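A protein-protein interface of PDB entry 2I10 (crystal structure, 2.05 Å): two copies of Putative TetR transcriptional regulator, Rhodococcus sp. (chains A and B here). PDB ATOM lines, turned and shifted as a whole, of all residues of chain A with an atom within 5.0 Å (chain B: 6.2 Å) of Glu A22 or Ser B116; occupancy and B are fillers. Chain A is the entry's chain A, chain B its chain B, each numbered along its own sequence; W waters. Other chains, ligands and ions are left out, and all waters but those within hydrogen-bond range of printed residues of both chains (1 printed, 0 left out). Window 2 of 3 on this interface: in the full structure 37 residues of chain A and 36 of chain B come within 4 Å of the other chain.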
ATOM      1  N   GLN A  18     -19.492  -0.343  -4.902  1.00  0.00           N
ATOM      2  CA  GLN A  18     -20.725  -0.146  -4.134  1.00  0.00           C
ATOM      3  C   GLN A  18     -21.949  -0.288  -5.051  1.00  0.00           C
ATOM      4  O   GLN A  18     -22.849  -1.067  -4.765  1.00  0.00           O
ATOM      5  CB  GLN A  18     -20.741   1.210  -3.428  1.00  0.00           C
ATOM      6  CG  GLN A  18     -21.977   1.384  -2.570  1.00  0.00           C
ATOM      7  CD  GLN A  18     -21.880   2.517  -1.553  1.00  0.00           C
ATOM      8  OE1 GLN A  18     -21.029   3.414  -1.640  1.00  0.00           O
ATOM      9  NE2 GLN A  18     -22.777   2.479  -0.575  1.00  0.00           N
ATOM     10  N   THR A  19     -21.964   0.425  -6.168  1.00  0.00           N
ATOM     11  CA  THR A  19     -23.103   0.362  -7.082  1.00  0.00           C
ATOM     12  C   THR A  19     -23.294  -1.049  -7.665  1.00  0.00           C
ATOM     13  O   THR A  19     -24.435  -1.498  -7.861  1.00  0.00           O
ATOM     14  CB  THR A  19     -22.951   1.352  -8.233  1.00  0.00           C
ATOM     15  OG1 THR A  19     -22.680   2.662  -7.713  1.00  0.00           O
ATOM     16  CG2 THR A  19     -24.235   1.391  -9.051  1.00  0.00           C
ATOM     17  N   ALA A  20     -22.178  -1.736  -7.928  1.00  0.00           N
ATOM     18  CA  ALA A  20     -22.199  -3.121  -8.418  1.00  0.00           C
ATOM     19  C   ALA A  20     -22.802  -4.030  -7.370  1.00  0.00           C
ATOM     20  O   ALA A  20     -23.665  -4.852  -7.679  1.00  0.00           O
ATOM     21  CB  ALA A  20     -20.782  -3.581  -8.805  1.00  0.00           C
ATOM     22  N   MET A  21     -22.380  -3.860  -6.120  1.00  0.00           N
ATOM     23  CA  MET A  21     -22.966  -4.626  -5.053  1.00  0.00           C
ATOM     24  C   MET A  21     -24.481  -4.442  -4.988  1.00  0.00           C
ATOM     25  O   MET A  21     -25.183  -5.429  -4.764  1.00  0.00           O
ATOM     26  CB  MET A  21     -22.321  -4.321  -3.709  1.00  0.00           C
ATOM     27  CG  MET A  21     -22.858  -5.194  -2.552  1.00  0.00           C
ATOM     28  SD  MET A  21     -22.169  -7.046  -2.658  1.00  0.00           S
ATOM     29  CE  MET A  21     -23.583  -7.998  -3.614  1.00  0.00           C
ATOM     30  N   GLU A  22     -24.971  -3.211  -5.199  1.00  0.00           N
ATOM     31  CA  GLU A  22     -26.412  -2.896  -5.105  1.00  0.00           C
ATOM     32  C   GLU A  22     -27.178  -3.668  -6.175  1.00  0.00           C
ATOM     33  O   GLU A  22     -28.204  -4.290  -5.897  1.00  0.00           O
ATOM     34  CB  GLU A  22     -26.707  -1.383  -5.255  1.00  0.00           C
ATOM     35  CG  GLU A  22     -26.285  -0.491  -4.086  1.00  0.00           C
ATOM     36  CD  GLU A  22     -26.447   1.025  -4.355  1.00  0.00           C
ATOM     37  OE1 GLU A  22     -26.674   1.448  -5.518  1.00  0.00           O
ATOM     38  OE2 GLU A  22     -26.328   1.808  -3.379  1.00  0.00           O
ATOM     39  N   LEU A  23     -26.665  -3.639  -7.395  1.00  0.00           N
ATOM     40  CA  LEU A  23     -27.266  -4.376  -8.501  1.00  0.00           C
ATOM     41  C   LEU A  23     -27.248  -5.895  -8.277  1.00  0.00           C
ATOM     42  O   LEU A  23     -28.241  -6.553  -8.537  1.00  0.00           O
ATOM     43  CB  LEU A  23     -26.543  -4.041  -9.801  1.00  0.00           C
ATOM     44  CG  LEU A  23     -27.249  -4.383 -11.105  1.00  0.00           C
ATOM     45  CD1 LEU A  23     -28.566  -3.636 -11.187  1.00  0.00           C
ATOM     46  CD2 LEU A  23     -26.367  -4.064 -12.333  1.00  0.00           C
ATOM     47  N   PHE A  24     -26.118  -6.447  -7.829  1.00  0.00           N
ATOM     48  CA  PHE A  24     -25.995  -7.894  -7.568  1.00  0.00           C
ATOM     49  C   PHE A  24     -26.930  -8.340  -6.426  1.00  0.00           C
ATOM     50  O   PHE A  24     -27.503  -9.444  -6.446  1.00  0.00           O
ATOM     51  CB  PHE A  24     -24.545  -8.266  -7.227  1.00  0.00           C
ATOM     52  CG  PHE A  24     -23.591  -8.288  -8.443  1.00  0.00           C
ATOM     53  CD1 PHE A  24     -23.963  -8.898  -9.640  1.00  0.00           C
ATOM     54  CD2 PHE A  24     -22.317  -7.714  -8.356  1.00  0.00           C
ATOM     55  CE1 PHE A  24     -23.099  -8.912 -10.730  1.00  0.00           C
ATOM     56  CE2 PHE A  24     -21.442  -7.764  -9.425  1.00  0.00           C
ATOM     57  CZ  PHE A  24     -21.833  -8.368 -10.620  1.00  0.00           C
ATOM     58  N   TRP A  25     -27.061  -7.492  -5.409  1.00  0.00           N
ATOM     59  CA  TRP A  25     -27.953  -7.778  -4.279  1.00  0.00           C
ATOM     60  C   TRP A  25     -29.386  -7.971  -4.773  1.00  0.00           C
ATOM     61  O   TRP A  25     -30.039  -8.918  -4.410  1.00  0.00           O
ATOM     62  CB  TRP A  25     -27.848  -6.666  -3.238  1.00  0.00           C
ATOM     63  CG  TRP A  25     -28.867  -6.690  -2.142  1.00  0.00           C
ATOM     64  CD1 TRP A  25     -30.116  -6.142  -2.172  1.00  0.00           C
ATOM     65  CD2 TRP A  25     -28.697  -7.235  -0.835  1.00  0.00           C
ATOM     66  NE1 TRP A  25     -30.750  -6.330  -0.969  1.00  0.00           N
ATOM     67  CE2 TRP A  25     -29.900  -6.985  -0.119  1.00  0.00           C
ATOM     68  CE3 TRP A  25     -27.648  -7.913  -0.188  1.00  0.00           C
ATOM     69  CZ2 TRP A  25     -30.097  -7.413   1.184  1.00  0.00           C
ATOM     70  CZ3 TRP A  25     -27.842  -8.321   1.144  1.00  0.00           C
ATOM     71  CH2 TRP A  25     -29.061  -8.073   1.801  1.00  0.00           C
ATOM     72  N   ARG A  26     -29.806  -7.112  -5.684  1.00  0.00           N
ATOM     73  CA  ARG A  26     -31.153  -7.122  -6.258  1.00  0.00           C
ATOM     74  C   ARG A  26     -31.382  -8.256  -7.289  1.00  0.00           C
ATOM     75  O   ARG A  26     -32.333  -9.047  -7.183  1.00  0.00           O
ATOM     76  CB  ARG A  26     -31.395  -5.727  -6.872  1.00  0.00           C
ATOM     77  CG  ARG A  26     -32.734  -5.470  -7.566  1.00  0.00           C
ATOM     78  CD  ARG A  26     -33.062  -3.940  -7.723  1.00  0.00           C
ATOM     79  NE  ARG A  26     -31.887  -3.062  -7.847  1.00  0.00           N
ATOM     80  CZ  ARG A  26     -31.395  -2.542  -8.978  1.00  0.00           C
ATOM     81  NH1 ARG A  26     -30.318  -1.762  -8.909  1.00  0.00           N
ATOM     82  NH2 ARG A  26     -31.952  -2.786 -10.172  1.00  0.00           N
ATOM     83  N   ALA A 115     -33.526  -0.673   3.450  1.00  0.00           N
ATOM     84  CA  ALA A 115     -33.517   0.194   2.253  1.00  0.00           C
ATOM     85  C   ALA A 115     -33.409  -0.572   0.930  1.00  0.00           C
ATOM     86  O   ALA A 115     -34.147  -0.291  -0.027  1.00  0.00           O
ATOM     87  CB  ALA A 115     -32.417   1.280   2.365  1.00  0.00           C
ATOM     88  N   SER A 116     -32.505  -1.551   0.880  1.00  0.00           N
ATOM     89  CA  SER A 116     -32.144  -2.220  -0.375  1.00  0.00           C
ATOM     90  C   SER A 116     -33.209  -3.164  -0.966  1.00  0.00           C
ATOM     91  O   SER A 116     -33.058  -3.630  -2.102  1.00  0.00           O
ATOM     92  CB  SER A 116     -30.819  -2.973  -0.216  1.00  0.00           C
ATOM     93  OG  SER A 116     -29.806  -2.142   0.327  1.00  0.00           O
ATOM     94  N   GLN B 111     -28.408  -2.415  10.596  1.00  0.00           N
ATOM     95  CA  GLN B 111     -28.891  -1.906   9.295  1.00  0.00           C
ATOM     96  C   GLN B 111     -28.155  -0.647   8.778  1.00  0.00           C
ATOM     97  O   GLN B 111     -27.767  -0.583   7.578  1.00  0.00           O
ATOM     98  CB  GLN B 111     -30.408  -1.661   9.381  1.00  0.00           C
ATOM     99  CG  GLN B 111     -31.213  -2.951   9.295  1.00  0.00           C
ATOM    100  CD  GLN B 111     -31.074  -3.611   7.909  1.00  0.00           C
ATOM    101  OE1 GLN B 111     -31.205  -2.929   6.883  1.00  0.00           O
ATOM    102  NE2 GLN B 111     -30.816  -4.941   7.878  1.00  0.00           N
ATOM    103  N   ALA B 112     -27.960   0.341   9.669  1.00  0.00           N
ATOM    104  CA  ALA B 112     -27.241   1.577   9.310  1.00  0.00           C
ATOM    105  C   ALA B 112     -25.781   1.319   8.922  1.00  0.00           C
ATOM    106  O   ALA B 112     -25.188   2.113   8.207  1.00  0.00           O
ATOM    107  CB  ALA B 112     -27.302   2.595  10.453  1.00  0.00           C
ATOM    108  N   GLY B 113     -25.215   0.207   9.399  1.00  0.00           N
ATOM    109  CA  GLY B 113     -23.811  -0.134   9.137  1.00  0.00           C
ATOM    110  C   GLY B 113     -23.582  -0.784   7.775  1.00  0.00           C
ATOM    111  O   GLY B 113     -22.425  -0.997   7.365  1.00  0.00           O
ATOM    112  N   LEU B 114     -24.666  -1.092   7.057  1.00  0.00           N
ATOM    113  CA  LEU B 114     -24.551  -1.705   5.721  1.00  0.00           C
ATOM    114  C   LEU B 114     -24.298  -0.620   4.640  1.00  0.00           C
ATOM    115  O   LEU B 114     -24.790   0.516   4.758  1.00  0.00           O
ATOM    116  CB  LEU B 114     -25.809  -2.545   5.400  1.00  0.00           C
ATOM    117  CG  LEU B 114     -26.264  -3.681   6.348  1.00  0.00           C
ATOM    118  CD1 LEU B 114     -27.765  -4.002   6.182  1.00  0.00           C
ATOM    119  CD2 LEU B 114     -25.452  -4.970   6.216  1.00  0.00           C
ATOM    120  N   ALA B 115     -23.510  -0.941   3.610  1.00  0.00           N
ATOM    121  CA  ALA B 115     -23.367  -0.015   2.472  1.00  0.00           C
ATOM    122  C   ALA B 115     -24.727   0.027   1.770  1.00  0.00           C
ATOM    123  O   ALA B 115     -25.355  -1.021   1.570  1.00  0.00           O
ATOM    124  CB  ALA B 115     -22.235  -0.440   1.516  1.00  0.00           C
ATOM    125  N   SER B 116     -25.189   1.236   1.444  1.00  0.00           N
ATOM    126  CA  SER B 116     -26.591   1.489   1.054  1.00  0.00           C
ATOM    127  C   SER B 116     -27.634   0.996   2.056  1.00  0.00           C
ATOM    128  O   SER B 116     -27.358   0.822   3.254  1.00  0.00           O
ATOM    129  CB  SER B 116     -26.906   0.909  -0.327  1.00  0.00           C
ATOM    130  OG  SER B 116     -28.313   0.761  -0.485  1.00  0.00           O
ATOM    131  N   PRO B 119     -30.657   5.022   5.618  1.00  0.00           N
ATOM    132  CA  PRO B 119     -31.650   5.630   6.544  1.00  0.00           C
ATOM    133  C   PRO B 119     -31.723   7.123   6.357  1.00  0.00           C
ATOM    134  O   PRO B 119     -30.708   7.764   6.074  1.00  0.00           O
ATOM    135  CB  PRO B 119     -31.095   5.325   7.945  1.00  0.00           C
ATOM    136  CG  PRO B 119     -29.593   5.128   7.726  1.00  0.00           C
ATOM    137  CD  PRO B 119     -29.435   4.583   6.316  1.00  0.00           C
HETATM  138  O   HOH W   1     -30.710  -0.814   5.272  1.00  0.00           O
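Of the 7 printed residues of chain B, 2 touch a printed residue of chain A. Hydrophobic or aromatic side chains of chain B within 4 Å of the printed part of chain A: Ala B115. Of the 11 printed residues of chain A, 3 touch a printed residue of chain B. Among the printed residues, 4 pairs touch across the chains.
Ser A116 touches its own counterpart, Ser B116. Of the 4 pairs that touch across the chains among the printed residues, 1 has its exchanged pair printed and touching as well.
N of Ser B116 sits close to NE2 of Gln A18 (3.4 Å). The side-chain hydroxyl of Ser A116 sits at hydrogen-bond distance from the side-chain hydroxyl of Ser B116, 3.4 Å away.
Ser B116 touches just these residues of chain A: Gln A18, Glu A22 and Ser A116. Of the printed residues of chain B, Gln A18 touches Ala B115 (3.6 Å) and Ser B116 (3.4 Å). Of the printed residues of chain B, Ser A116 touches Ser B116 (3.4 Å). Printed residues of chain A within 4 Å of Ala B115: Gln A18. Pro B119 touches none of the printed residues of chain A. The nearest residue of chain A that does not touch Ser B116 is Ala A115 (4.8 Å). The nearest printed residue of chain A that does not touch Ala B115 is Ser A116 (4.8 Å).
Gln A18 touches Ala B115. Glu A22 touches Ser B116 (OE2 to CB, 3.2 Å).
Water W1 lies within hydrogen-bond range of OE1 of Gln B111 and N of Ala A115.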
